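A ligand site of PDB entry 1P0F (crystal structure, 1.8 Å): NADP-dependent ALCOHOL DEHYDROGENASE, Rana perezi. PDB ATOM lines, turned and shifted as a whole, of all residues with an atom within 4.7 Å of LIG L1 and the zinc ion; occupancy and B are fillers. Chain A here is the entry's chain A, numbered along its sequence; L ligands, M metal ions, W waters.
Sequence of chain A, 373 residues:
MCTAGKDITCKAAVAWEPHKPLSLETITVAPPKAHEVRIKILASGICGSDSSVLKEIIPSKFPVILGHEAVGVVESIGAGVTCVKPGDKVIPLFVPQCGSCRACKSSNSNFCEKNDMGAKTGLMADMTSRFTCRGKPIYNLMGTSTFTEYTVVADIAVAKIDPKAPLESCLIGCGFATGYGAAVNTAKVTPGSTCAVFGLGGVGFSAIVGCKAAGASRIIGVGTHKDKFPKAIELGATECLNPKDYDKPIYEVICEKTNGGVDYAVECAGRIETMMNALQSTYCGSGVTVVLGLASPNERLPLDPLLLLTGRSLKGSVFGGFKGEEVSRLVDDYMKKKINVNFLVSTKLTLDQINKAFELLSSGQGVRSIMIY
The side-chain sulfur (SG) of Cys 47 sits close to an oxygen (O9) of LIG L1, at 3.4 Å.
An oxygen (O15) of LIG L1 is in hydrogen-bond range of a ring nitrogen (ND1) of His 225 (2.7 Å).
N of Gly 202 is in hydrogen-bond range of O2 of LIG L1 (3.4 Å).
An oxygen (O15) of LIG L1 is in salt-bridge range of the side-chain amino group (NZ) of Lys 228, 3.3 Å away.
O17 of LIG L1 is in hydrogen-bond range of OG1 of Thr 224 (2.9 Å).
The backbone NH of Thr 224 is in hydrogen-bond range of an oxygen (O17) of LIG L1 (2.9 Å).
A nitrogen (N7) of LIG L1 lies within hydrogen-bond range of the backbone carbonyl oxygen (O) of Ser 317 (3.1 Å).
N7 of LIG L1 lies close to O of Leu 292 (3.2 Å).
N of Leu 200 lies within hydrogen-bond range of O16 of LIG L1 (2.8 Å).
N of Val 203 sits at hydrogen-bond distance from O8 of LIG L1 (2.9 Å).
The backbone NH of Gly 201 lies close to an oxygen (O5) of LIG L1.
An oxygen (O14) of LIG L1 lies within hydrogen-bond range of the backbone NH of Phe 319 (2.8 Å).
The backbone NH of Leu 294 sits at hydrogen-bond distance from an oxygen (O12) of LIG L1 (3.3 Å).
The backbone NH (N) of Gly 48 is in hydrogen-bond range of an oxygen (O9) of LIG L1 (2.8 Å).
OG of Ser 49 lies within hydrogen-bond range of O13 of LIG L1 (2.8 Å).
The guanidinium group (NH1) of Arg 368 is in salt-bridge range of an oxygen (O9) of LIG L1 (3.1 Å).
OG1 of Thr 178 sits close to O14 of LIG L1 (3.4 Å).
OE1 of Glu 69 is in salt-bridge range of NE of Arg 368, 2.7 Å away.
OG1 of Thr 178 lies within hydrogen-bond range of O of Cys 174 (2.7 Å).
The side-chain hydroxyl of Ser 52 sits at hydrogen-bond distance from the backbone carbonyl oxygen of Gly 48 (3.3 Å).
The side-chain hydroxyl (OG1) of Thr 224 lies within hydrogen-bond range of a ring nitrogen (ND1) of His 225 (3.1 Å).
N of Ser 49 sits close to SG of Cys 47 (3.3 Å).
SG of Cys 47 lies close to NH2 of Arg 368 (3.5 Å).
The backbone carbonyl oxygen of Val 222 lies within hydrogen-bond range of the backbone NH of Gly 199.
NZ of Lys 228 lies within hydrogen-bond range of O of Leu 200 (3.1 Å).
The guanidinium group (NE) of Arg 271 lies close to a nitrogen (N3) of LIG L1, at 3.3 Å.
Merely in contact with LIG L1: Gly 199, Gly 223, Cys 268, Ala 269, Gly 270, Gly 293, Val 318 and Leu 361.
Hydrophobic or aromatic side chains that line LIG L1: Leu 200, Val 203, His 225, Ala 269, Leu 294, Val 318 and Leu 361.
Ser 49 touches the zinc ion.
Of the 35 residues printed, 4 come within 4 Å of the zinc ion.
The nearest printed residue that does not touch the zinc ion is Glu 69 (4.6 Å).
SG of Cys 174 is bound to the zinc ion, 2.3 Å away.
NE2 of His 68 binds the zinc ion (2.3 Å).
The side-chain sulfur (SG) of Cys 47 is bound to the zinc ion (2.4 Å).
Slightly farther from the zinc ion lies an oxygen (O1) of LG2 L2 (2.8 Å).
Water W2 lies within hydrogen-bond range of an oxygen (O16) of LIG L1 (2.7 Å), the backbone NH of His 225 (2.8 Å) and the backbone NH of Thr 224 (3.4 Å).
Water W6 bridges an oxygen (O12) of LIG L1 (2.7 Å) and the backbone carbonyl oxygen (O) of Ala 269 (3.1 Å).
Water W8 lies within hydrogen-bond range of OG of Ser 52, O of Leu 294 and O13 of LIG L1.
Water W7 lies within hydrogen-bond range of O of Val 367 (2.5 Å), O2 of LIG L1 (2.9 Å) and NH1 of Arg 368 (2.9 Å).
Water W1 lies within hydrogen-bond range of an oxygen (O2) of LIG L1 and the backbone carbonyl oxygen (O) of Val 367.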
ATOM      1  N   CYS A  47       0.325  18.971  19.240  1.00  0.00           N
ATOM      2  CA  CYS A  47       1.108  18.693  18.046  1.00  0.00           C
ATOM      3  C   CYS A  47       2.104  17.548  18.206  1.00  0.00           C
ATOM      4  O   CYS A  47       2.587  17.281  19.307  1.00  0.00           O
ATOM      5  CB  CYS A  47       1.860  19.962  17.622  1.00  0.00           C
ATOM      6  SG  CYS A  47       2.935  19.762  16.198  1.00  0.00           S
ATOM      7  N   GLY A  48       2.400  16.883  17.104  1.00  0.00           N
ATOM      8  CA  GLY A  48       3.354  15.785  17.141  1.00  0.00           C
ATOM      9  C   GLY A  48       4.672  16.252  17.736  1.00  0.00           C
ATOM     10  O   GLY A  48       5.379  15.475  18.373  1.00  0.00           O
ATOM     11  N   SER A  49       5.015  17.521  17.526  1.00  0.00           N
ATOM     12  CA  SER A  49       6.259  18.050  18.068  1.00  0.00           C
ATOM     13  C   SER A  49       6.220  18.082  19.587  1.00  0.00           C
ATOM     14  O   SER A  49       7.249  17.898  20.237  1.00  0.00           O
ATOM     15  CB  SER A  49       6.522  19.456  17.522  1.00  0.00           C
ATOM     16  OG  SER A  49       6.798  19.390  16.136  1.00  0.00           O
ATOM     17  N   SER A  52       7.101  14.713  20.576  1.00  0.00           N
ATOM     18  CA  SER A  52       8.520  14.465  20.344  1.00  0.00           C
ATOM     19  C   SER A  52       9.398  15.026  21.453  1.00  0.00           C
ATOM     20  O   SER A  52      10.422  14.425  21.800  1.00  0.00           O
ATOM     21  CB  SER A  52       8.945  15.029  18.984  1.00  0.00           C
ATOM     22  OG  SER A  52       8.418  14.218  17.944  1.00  0.00           O
ATOM     23  N   ILE A  58      12.989  15.714  20.214  1.00  0.00           N
ATOM     24  CA  ILE A  58      13.315  17.122  20.061  1.00  0.00           C
ATOM     25  C   ILE A  58      13.813  17.566  21.434  1.00  0.00           C
ATOM     26  O   ILE A  58      13.100  17.445  22.430  1.00  0.00           O
ATOM     27  CB  ILE A  58      12.075  17.976  19.724  1.00  0.00           C
ATOM     28  CG1 ILE A  58      11.512  17.577  18.346  1.00  0.00           C
ATOM     29  CG2 ILE A  58      12.438  19.455  19.747  1.00  0.00           C
ATOM     30  CD1 ILE A  58      10.234  18.301  17.984  1.00  0.00           C
ATOM     31  N   HIS A  68       2.300  24.754  21.555  1.00  0.00           N
ATOM     32  CA  HIS A  68       2.693  25.898  20.753  1.00  0.00           C
ATOM     33  C   HIS A  68       1.692  26.131  19.631  1.00  0.00           C
ATOM     34  O   HIS A  68       1.992  26.791  18.639  1.00  0.00           O
ATOM     35  CB  HIS A  68       4.088  25.669  20.155  1.00  0.00           C
ATOM     36  CG  HIS A  68       4.212  24.367  19.444  1.00  0.00           C
ATOM     37  ND1 HIS A  68       4.200  23.152  20.099  1.00  0.00           N
ATOM     38  CD2 HIS A  68       4.328  24.078  18.123  1.00  0.00           C
ATOM     39  CE1 HIS A  68       4.311  22.174  19.217  1.00  0.00           C
ATOM     40  NE2 HIS A  68       4.384  22.710  18.005  1.00  0.00           N
ATOM     41  N   GLU A  69       0.501  25.589  19.813  1.00  0.00           N
ATOM     42  CA  GLU A  69      -0.561  25.684  18.811  1.00  0.00           C
ATOM     43  C   GLU A  69      -1.821  26.189  19.510  1.00  0.00           C
ATOM     44  O   GLU A  69      -2.571  25.399  20.074  1.00  0.00           O
ATOM     45  CB  GLU A  69      -0.785  24.281  18.247  1.00  0.00           C
ATOM     46  CG  GLU A  69      -1.493  24.176  16.922  1.00  0.00           C
ATOM     47  CD  GLU A  69      -1.547  22.733  16.422  1.00  0.00           C
ATOM     48  OE1 GLU A  69      -2.372  21.955  16.932  1.00  0.00           O
ATOM     49  OE2 GLU A  69      -0.737  22.378  15.535  1.00  0.00           O
ATOM     50  N   PHE A  94       5.430  30.573  17.439  1.00  0.00           N
ATOM     51  CA  PHE A  94       6.624  29.885  17.918  1.00  0.00           C
ATOM     52  C   PHE A  94       7.829  30.268  17.052  1.00  0.00           C
ATOM     53  O   PHE A  94       8.974  30.019  17.412  1.00  0.00           O
ATOM     54  CB  PHE A  94       6.398  28.368  17.989  1.00  0.00           C
ATOM     55  CG  PHE A  94       6.261  27.689  16.660  1.00  0.00           C
ATOM     56  CD1 PHE A  94       7.385  27.221  15.991  1.00  0.00           C
ATOM     57  CD2 PHE A  94       5.006  27.482  16.107  1.00  0.00           C
ATOM     58  CE1 PHE A  94       7.243  26.545  14.772  1.00  0.00           C
ATOM     59  CE2 PHE A  94       4.868  26.798  14.893  1.00  0.00           C
ATOM     60  CZ  PHE A  94       5.993  26.336  14.232  1.00  0.00           C
ATOM     61  N   CYS A 174       0.113  26.235  14.280  1.00  0.00           N
ATOM     62  CA  CYS A 174       1.198  25.347  13.884  1.00  0.00           C
ATOM     63  C   CYS A 174       0.859  24.305  12.826  1.00  0.00           C
ATOM     64  O   CYS A 174       1.219  24.443  11.663  1.00  0.00           O
ATOM     65  CB  CYS A 174       1.791  24.610  15.075  1.00  0.00           C
ATOM     66  SG  CYS A 174       3.201  23.635  14.519  1.00  0.00           S
ATOM     67  N   THR A 178       1.626  24.849   8.859  1.00  0.00           N
ATOM     68  CA  THR A 178       2.764  24.058   8.422  1.00  0.00           C
ATOM     69  C   THR A 178       2.464  23.196   7.206  1.00  0.00           C
ATOM     70  O   THR A 178       3.141  23.284   6.180  1.00  0.00           O
ATOM     71  CB  THR A 178       3.271  23.151   9.552  1.00  0.00           C
ATOM     72  OG1 THR A 178       3.699  23.972  10.656  1.00  0.00           O
ATOM     73  CG2 THR A 178       4.427  22.291   9.071  1.00  0.00           C
ATOM     74  N   GLY A 199       2.344  10.423   5.565  1.00  0.00           N
ATOM     75  CA  GLY A 199       2.059  10.637   6.976  1.00  0.00           C
ATOM     76  C   GLY A 199       0.773  11.431   7.085  1.00  0.00           C
ATOM     77  O   GLY A 199       0.779  12.651   6.935  1.00  0.00           O
ATOM     78  N   LEU A 200      -0.326  10.746   7.358  1.00  0.00           N
ATOM     79  CA  LEU A 200      -1.617  11.401   7.442  1.00  0.00           C
ATOM     80  C   LEU A 200      -2.030  11.860   8.835  1.00  0.00           C
ATOM     81  O   LEU A 200      -3.047  11.420   9.378  1.00  0.00           O
ATOM     82  CB  LEU A 200      -2.693  10.495   6.837  1.00  0.00           C
ATOM     83  CG  LEU A 200      -2.400  10.024   5.404  1.00  0.00           C
ATOM     84  CD1 LEU A 200      -3.554   9.177   4.887  1.00  0.00           C
ATOM     85  CD2 LEU A 200      -2.172  11.226   4.500  1.00  0.00           C
ATOM     86  N   GLY A 201      -1.229  12.751   9.413  1.00  0.00           N
ATOM     87  CA  GLY A 201      -1.535  13.292  10.727  1.00  0.00           C
ATOM     88  C   GLY A 201      -2.043  14.707  10.568  1.00  0.00           C
ATOM     89  O   GLY A 201      -2.555  15.067   9.496  1.00  0.00           O
ATOM     90  N   GLY A 202      -1.923  15.517  11.613  1.00  0.00           N
ATOM     91  CA  GLY A 202      -2.388  16.892  11.523  1.00  0.00           C
ATOM     92  C   GLY A 202      -1.727  17.647  10.385  1.00  0.00           C
ATOM     93  O   GLY A 202      -2.393  18.325   9.597  1.00  0.00           O
ATOM     94  N   VAL A 203      -0.409  17.536  10.304  1.00  0.00           N
ATOM     95  CA  VAL A 203       0.339  18.215   9.249  1.00  0.00           C
ATOM     96  C   VAL A 203       0.032  17.615   7.878  1.00  0.00           C
ATOM     97  O   VAL A 203      -0.178  18.347   6.915  1.00  0.00           O
ATOM     98  CB  VAL A 203       1.861  18.156   9.530  1.00  0.00           C
ATOM     99  CG1 VAL A 203       2.640  18.690   8.334  1.00  0.00           C
ATOM    100  CG2 VAL A 203       2.178  18.983  10.779  1.00  0.00           C
ATOM    101  N   GLY A 204      -0.011  16.284   7.805  1.00  0.00           N
ATOM    102  CA  GLY A 204      -0.299  15.623   6.547  1.00  0.00           C
ATOM    103  C   GLY A 204      -1.627  16.049   5.945  1.00  0.00           C
ATOM    104  O   GLY A 204      -1.709  16.378   4.761  1.00  0.00           O
ATOM    105  N   VAL A 222      -0.422   8.848   1.563  1.00  0.00           N
ATOM    106  CA  VAL A 222       0.300   7.629   1.884  1.00  0.00           C
ATOM    107  C   VAL A 222       0.469   7.503   3.390  1.00  0.00           C
ATOM    108  O   VAL A 222       1.111   8.332   4.034  1.00  0.00           O
ATOM    109  CB  VAL A 222       1.706   7.627   1.226  1.00  0.00           C
ATOM    110  CG1 VAL A 222       2.430   6.315   1.536  1.00  0.00           C
ATOM    111  CG2 VAL A 222       1.566   7.829  -0.277  1.00  0.00           C
ATOM    112  N   GLY A 223      -0.122   6.445   3.955  1.00  0.00           N
ATOM    113  CA  GLY A 223      -0.046   6.210   5.384  1.00  0.00           C
ATOM    114  C   GLY A 223      -0.294   4.751   5.729  1.00  0.00           C
ATOM    115  O   GLY A 223      -0.768   3.985   4.893  1.00  0.00           O
ATOM    116  N   THR A 224       0.003   4.371   6.974  1.00  0.00           N
ATOM    117  CA  THR A 224      -0.182   2.997   7.419  1.00  0.00           C
ATOM    118  C   THR A 224      -1.528   2.730   8.101  1.00  0.00           C
ATOM    119  O   THR A 224      -1.768   1.616   8.564  1.00  0.00           O
ATOM    120  CB  THR A 224       0.935   2.583   8.406  1.00  0.00           C
ATOM    121  OG1 THR A 224       0.961   3.492   9.515  1.00  0.00           O
ATOM    122  CG2 THR A 224       2.291   2.599   7.710  1.00  0.00           C
ATOM    123  N   HIS A 225      -2.391   3.731   8.147  1.00  0.00           N
ATOM    124  CA  HIS A 225      -3.698   3.560   8.779  1.00  0.00           C
ATOM    125  C   HIS A 225      -4.838   3.856   7.816  1.00  0.00           C
ATOM    126  O   HIS A 225      -5.292   4.992   7.691  1.00  0.00           O
ATOM    127  CB  HIS A 225      -3.810   4.436  10.028  1.00  0.00           C
ATOM    128  CG  HIS A 225      -2.812   4.102  11.085  1.00  0.00           C
ATOM    129  ND1 HIS A 225      -1.519   4.572  11.065  1.00  0.00           N
ATOM    130  CD2 HIS A 225      -2.889   3.290  12.168  1.00  0.00           C
ATOM    131  CE1 HIS A 225      -0.847   4.073  12.086  1.00  0.00           C
ATOM    132  NE2 HIS A 225      -1.664   3.292  12.770  1.00  0.00           N
ATOM    133  N   LYS A 228      -8.038   6.171   8.022  1.00  0.00           N
ATOM    134  CA  LYS A 228      -7.981   7.617   7.802  1.00  0.00           C
ATOM    135  C   LYS A 228      -8.218   8.012   6.336  1.00  0.00           C
ATOM    136  O   LYS A 228      -8.490   9.184   6.046  1.00  0.00           O
ATOM    137  CB  LYS A 228      -6.616   8.176   8.212  1.00  0.00           C
ATOM    138  CG  LYS A 228      -6.278   8.061   9.685  1.00  0.00           C
ATOM    139  CD  LYS A 228      -4.918   8.700   9.942  1.00  0.00           C
ATOM    140  CE  LYS A 228      -4.533   8.658  11.404  1.00  0.00           C
ATOM    141  NZ  LYS A 228      -3.202   9.291  11.608  1.00  0.00           N
ATOM    142  N   CYS A 268       5.563  14.134   6.204  1.00  0.00           N
ATOM    143  CA  CYS A 268       4.968  14.666   7.427  1.00  0.00           C
ATOM    144  C   CYS A 268       4.949  13.669   8.575  1.00  0.00           C
ATOM    145  O   CYS A 268       4.077  13.738   9.438  1.00  0.00           O
ATOM    146  CB  CYS A 268       3.516  15.083   7.142  1.00  0.00           C
ATOM    147  SG  CYS A 268       3.269  16.104   5.679  1.00  0.00           S
ATOM    148  N   ALA A 269       5.908  12.750   8.600  1.00  0.00           N
ATOM    149  CA  ALA A 269       5.934  11.743   9.658  1.00  0.00           C
ATOM    150  C   ALA A 269       7.120  11.863  10.607  1.00  0.00           C
ATOM    151  O   ALA A 269       7.033  11.477  11.770  1.00  0.00           O
ATOM    152  CB  ALA A 269       5.909  10.343   9.048  1.00  0.00           C
ATOM    153  N   GLY A 270       8.222  12.403  10.113  1.00  0.00           N
ATOM    154  CA  GLY A 270       9.404  12.551  10.945  1.00  0.00           C
ATOM    155  C   GLY A 270      10.213  11.268  11.019  1.00  0.00           C
ATOM    156  O   GLY A 270      10.757  10.937  12.077  1.00  0.00           O
ATOM    157  N   ARG A 271      10.282  10.530   9.907  1.00  0.00           N
ATOM    158  CA  ARG A 271      11.031   9.270   9.855  1.00  0.00           C
ATOM    159  C   ARG A 271      11.945   9.276   8.634  1.00  0.00           C
ATOM    160  O   ARG A 271      11.519   9.644   7.538  1.00  0.00           O
ATOM    161  CB  ARG A 271      10.081   8.081   9.762  1.00  0.00           C
ATOM    162  CG  ARG A 271       9.029   8.010  10.862  1.00  0.00           C
ATOM    163  CD  ARG A 271       9.655   8.014  12.238  1.00  0.00           C
ATOM    164  NE  ARG A 271       8.650   7.963  13.300  1.00  0.00           N
ATOM    165  CZ  ARG A 271       8.922   8.050  14.600  1.00  0.00           C
ATOM    166  NH1 ARG A 271      10.180   8.196  15.008  1.00  0.00           N
ATOM    167  NH2 ARG A 271       7.934   7.990  15.491  1.00  0.00           N
ATOM    168  N   LEU A 292       9.199  17.910   6.445  1.00  0.00           N
ATOM    169  CA  LEU A 292       8.673  18.730   7.528  1.00  0.00           C
ATOM    170  C   LEU A 292       8.877  18.087   8.889  1.00  0.00           C
ATOM    171  O   LEU A 292       9.028  18.777   9.898  1.00  0.00           O
ATOM    172  CB  LEU A 292       7.177  18.970   7.326  1.00  0.00           C
ATOM    173  CG  LEU A 292       6.731  19.626   6.023  1.00  0.00           C
ATOM    174  CD1 LEU A 292       5.208  19.595   5.964  1.00  0.00           C
ATOM    175  CD2 LEU A 292       7.253  21.063   5.953  1.00  0.00           C
ATOM    176  N   GLY A 293       8.870  16.757   8.918  1.00  0.00           N
ATOM    177  CA  GLY A 293       9.042  16.040  10.177  1.00  0.00           C
ATOM    178  C   GLY A 293      10.449  16.073  10.729  1.00  0.00           C
ATOM    179  O   GLY A 293      11.418  16.246   9.999  1.00  0.00           O
ATOM    180  N   LEU A 294      10.558  15.925  12.054  1.00  0.00           N
ATOM    181  CA  LEU A 294      11.855  15.923  12.705  1.00  0.00           C
ATOM    182  C   LEU A 294      12.130  14.530  13.282  1.00  0.00           C
ATOM    183  O   LEU A 294      11.358  14.024  14.087  1.00  0.00           O
ATOM    184  CB  LEU A 294      11.905  16.963  13.829  1.00  0.00           C
ATOM    185  CG  LEU A 294      11.826  18.445  13.455  1.00  0.00           C
ATOM    186  CD1 LEU A 294      10.434  18.780  12.930  1.00  0.00           C
ATOM    187  CD2 LEU A 294      12.159  19.296  14.671  1.00  0.00           C
ATOM    188  N   SER A 317      11.275  23.367   5.641  1.00  0.00           N
ATOM    189  CA  SER A 317      10.843  24.656   6.146  1.00  0.00           C
ATOM    190  C   SER A 317      10.142  24.471   7.479  1.00  0.00           C
ATOM    191  O   SER A 317       9.790  23.350   7.861  1.00  0.00           O
ATOM    192  CB  SER A 317       9.865  25.317   5.168  1.00  0.00           C
ATOM    193  OG  SER A 317       8.631  24.615   5.112  1.00  0.00           O
ATOM    194  N   VAL A 318       9.963  25.574   8.204  1.00  0.00           N
ATOM    195  CA  VAL A 318       9.267  25.555   9.483  1.00  0.00           C
ATOM    196  C   VAL A 318       8.029  26.441   9.322  1.00  0.00           C
ATOM    197  O   VAL A 318       8.044  27.395   8.537  1.00  0.00           O
ATOM    198  CB  VAL A 318      10.135  26.122  10.628  1.00  0.00           C
ATOM    199  CG1 VAL A 318       9.275  26.322  11.867  1.00  0.00           C
ATOM    200  CG2 VAL A 318      11.279  25.168  10.944  1.00  0.00           C
ATOM    201  N   PHE A 319       6.970  26.125  10.060  1.00  0.00           N
ATOM    202  CA  PHE A 319       5.725  26.886  10.023  1.00  0.00           C
ATOM    203  C   PHE A 319       5.229  27.126   8.597  1.00  0.00           C
ATOM    204  O   PHE A 319       4.667  28.181   8.305  1.00  0.00           O
ATOM    205  CB  PHE A 319       5.915  28.216  10.756  1.00  0.00           C
ATOM    206  CG  PHE A 319       4.621  28.892  11.146  1.00  0.00           C
ATOM    207  CD1 PHE A 319       4.423  30.247  10.886  1.00  0.00           C
ATOM    208  CD2 PHE A 319       3.618  28.173  11.792  1.00  0.00           C
ATOM    209  CE1 PHE A 319       3.232  30.871  11.265  1.00  0.00           C
ATOM    210  CE2 PHE A 319       2.430  28.789  12.176  1.00  0.00           C
ATOM    211  CZ  PHE A 319       2.228  30.152  11.911  1.00  0.00           C
ATOM    212  N   GLY A 320       5.454  26.142   7.731  1.00  0.00           N
ATOM    213  CA  GLY A 320       5.013  26.219   6.344  1.00  0.00           C
ATOM    214  C   GLY A 320       5.536  27.376   5.517  1.00  0.00           C
ATOM    215  O   GLY A 320       4.974  27.709   4.474  1.00  0.00           O
ATOM    216  N   LEU A 361      -2.311  10.132  19.511  1.00  0.00           N
ATOM    217  CA  LEU A 361      -1.334  10.269  18.446  1.00  0.00           C
ATOM    218  C   LEU A 361      -0.813   8.884  18.049  1.00  0.00           C
ATOM    219  O   LEU A 361      -0.296   8.702  16.948  1.00  0.00           O
ATOM    220  CB  LEU A 361      -0.165  11.147  18.901  1.00  0.00           C
ATOM    221  CG  LEU A 361      -0.513  12.612  19.191  1.00  0.00           C
ATOM    222  CD1 LEU A 361       0.723  13.340  19.722  1.00  0.00           C
ATOM    223  CD2 LEU A 361      -1.018  13.278  17.906  1.00  0.00           C
ATOM    224  N   VAL A 367      -7.453  13.043  13.268  1.00  0.00           N
ATOM    225  CA  VAL A 367      -6.402  13.926  12.783  1.00  0.00           C
ATOM    226  C   VAL A 367      -5.799  14.737  13.917  1.00  0.00           C
ATOM    227  O   VAL A 367      -4.701  14.422  14.383  1.00  0.00           O
ATOM    228  CB  VAL A 367      -6.971  14.885  11.718  1.00  0.00           C
ATOM    229  CG1 VAL A 367      -5.867  15.780  11.176  1.00  0.00           C
ATOM    230  CG2 VAL A 367      -7.596  14.078  10.586  1.00  0.00           C
ATOM    231  N   ARG A 368      -6.517  15.750  14.379  1.00  0.00           N
ATOM    232  CA  ARG A 368      -6.040  16.612  15.457  1.00  0.00           C
ATOM    233  C   ARG A 368      -6.958  16.660  16.666  1.00  0.00           C
ATOM    234  O   ARG A 368      -8.191  16.618  16.538  1.00  0.00           O
ATOM    235  CB  ARG A 368      -5.849  18.041  14.936  1.00  0.00           C
ATOM    236  CG  ARG A 368      -4.413  18.452  14.616  1.00  0.00           C
ATOM    237  CD  ARG A 368      -3.658  18.824  15.883  1.00  0.00           C
ATOM    238  NE  ARG A 368      -2.422  19.556  15.597  1.00  0.00           N
ATOM    239  CZ  ARG A 368      -1.330  19.014  15.072  1.00  0.00           C
ATOM    240  NH1 ARG A 368      -1.309  17.721  14.773  1.00  0.00           N
ATOM    241  NH2 ARG A 368      -0.261  19.759  14.838  1.00  0.00           N
HETATM  242  P1  LIG L   1       1.001  13.364  14.248  1.00  0.00           P
HETATM  243  O1  LIG L   1       1.537  12.532  15.257  1.00  0.00           O
HETATM  244  O2  LIG L   1      -0.390  14.004  14.253  1.00  0.00           O
HETATM  245  O3  LIG L   1       1.054  12.614  12.839  1.00  0.00           O
HETATM  246  C1  LIG L   1       2.294  12.042  12.351  1.00  0.00           C
HETATM  247  C2  LIG L   1       1.755  11.121  11.279  1.00  0.00           C
HETATM  248  O4  LIG L   1       2.933  10.477  10.608  1.00  0.00           O
HETATM  249  C3  LIG L   1       0.939   9.905  11.792  1.00  0.00           C
HETATM  250  O5  LIG L   1      -0.444  10.263  11.669  1.00  0.00           O
HETATM  251  C4  LIG L   1       1.367   8.773  10.872  1.00  0.00           C
HETATM  252  O6  LIG L   1       0.659   8.740   9.645  1.00  0.00           O
HETATM  253  C5  LIG L   1       2.865   9.068  10.606  1.00  0.00           C
HETATM  254  N1  LIG L   1       3.722   8.410  11.609  1.00  0.00           N
HETATM  255  C6  LIG L   1       4.025   8.707  12.930  1.00  0.00           C
HETATM  256  N2  LIG L   1       4.861   7.852  13.494  1.00  0.00           N
HETATM  257  C7  LIG L   1       5.127   6.943  12.480  1.00  0.00           C
HETATM  258  C8  LIG L   1       5.949   5.795  12.482  1.00  0.00           C
HETATM  259  N3  LIG L   1       6.691   5.325  13.505  1.00  0.00           N
HETATM  260  N4  LIG L   1       6.021   5.056  11.284  1.00  0.00           N
HETATM  261  C9  LIG L   1       5.296   5.453  10.148  1.00  0.00           C
HETATM  262  N5  LIG L   1       4.470   6.570  10.117  1.00  0.00           N
HETATM  263  C10 LIG L   1       4.421   7.291  11.311  1.00  0.00           C
HETATM  264  O7  LIG L   1       1.953  14.602  14.009  1.00  0.00           O
HETATM  265  P2  LIG L   1       1.575  15.989  13.409  1.00  0.00           P
HETATM  266  O8  LIG L   1       1.489  16.184  11.961  1.00  0.00           O
HETATM  267  O9  LIG L   1       1.721  17.103  14.387  1.00  0.00           O
HETATM  268  O10 LIG L   1       3.204  16.089  13.162  1.00  0.00           O
HETATM  269  C11 LIG L   1       3.939  15.208  12.210  1.00  0.00           C
HETATM  270  C12 LIG L   1       5.420  15.564  12.079  1.00  0.00           C
HETATM  271  O11 LIG L   1       5.622  16.936  11.619  1.00  0.00           O
HETATM  272  C13 LIG L   1       6.320  15.442  13.370  1.00  0.00           C
HETATM  273  O12 LIG L   1       7.571  14.794  13.055  1.00  0.00           O
HETATM  274  C14 LIG L   1       6.480  16.890  13.805  1.00  0.00           C
HETATM  275  O13 LIG L   1       7.615  17.120  14.641  1.00  0.00           O
HETATM  276  C15 LIG L   1       6.589  17.588  12.510  1.00  0.00           C
HETATM  277  N6  LIG L   1       6.210  19.029  12.453  1.00  0.00           N
HETATM  278  C16 LIG L   1       6.982  19.963  11.724  1.00  0.00           C
HETATM  279  C17 LIG L   1       6.574  21.296  11.711  1.00  0.00           C
HETATM  280  C18 LIG L   1       7.410  22.313  10.935  1.00  0.00           C
HETATM  281  O14 LIG L   1       7.037  23.473  10.959  1.00  0.00           O
HETATM  282  N7  LIG L   1       8.474  21.933  10.267  1.00  0.00           N
HETATM  283  C19 LIG L   1       5.371  21.733  12.444  1.00  0.00           C
HETATM  284  C20 LIG L   1       4.625  20.754  13.162  1.00  0.00           C
HETATM  285  C21 LIG L   1       5.021  19.382  13.179  1.00  0.00           C
HETATM  286  P3  LIG L   1      -0.197   7.457   9.128  1.00  0.00           P
HETATM  287  O15 LIG L   1      -1.156   7.092  10.272  1.00  0.00           O
HETATM  288  O16 LIG L   1      -0.877   8.024   7.937  1.00  0.00           O
HETATM  289  O17 LIG L   1       0.805   6.346   8.867  1.00  0.00           O
HETATM  290  C1  LG2 L   2       7.963  21.961  15.141  1.00  0.00           C
HETATM  291  O1  LG2 L   2       6.667  22.212  15.665  1.00  0.00           O
HETATM  292  C2  LG2 L   2       9.040  22.751  15.838  1.00  0.00           C
HETATM  293  O2  LG2 L   2       9.833  23.433  14.882  1.00  0.00           O
HETATM  294  C3  LG2 L   2       9.884  21.808  16.682  1.00  0.00           C
HETATM  295  O3  LG2 L   2      10.933  22.489  17.362  1.00  0.00           O
HETATM  296 ZN    ZN M   1       3.865  21.982  15.905  1.00  0.00          ZN
HETATM  297  O   HOH W   1      -2.705  11.908  14.201  1.00  0.00           O
HETATM  298  O   HOH W   2      -2.805   6.364   7.141  1.00  0.00           O
HETATM  299  O   HOH W   3       1.108  14.500   9.736  1.00  0.00           O
HETATM  300  O   HOH W   4       3.165   6.888   7.695  1.00  0.00           O
HETATM  301  O   HOH W   5       3.568  12.071  16.912  1.00  0.00           O
HETATM  302  O   HOH W   6       7.670  12.593  14.563  1.00  0.00           O
HETATM  303  O   HOH W   7      -2.620  15.268  15.571  1.00  0.00           O
HETATM  304  O   HOH W   8       9.456  15.264  15.682  1.00  0.00           O
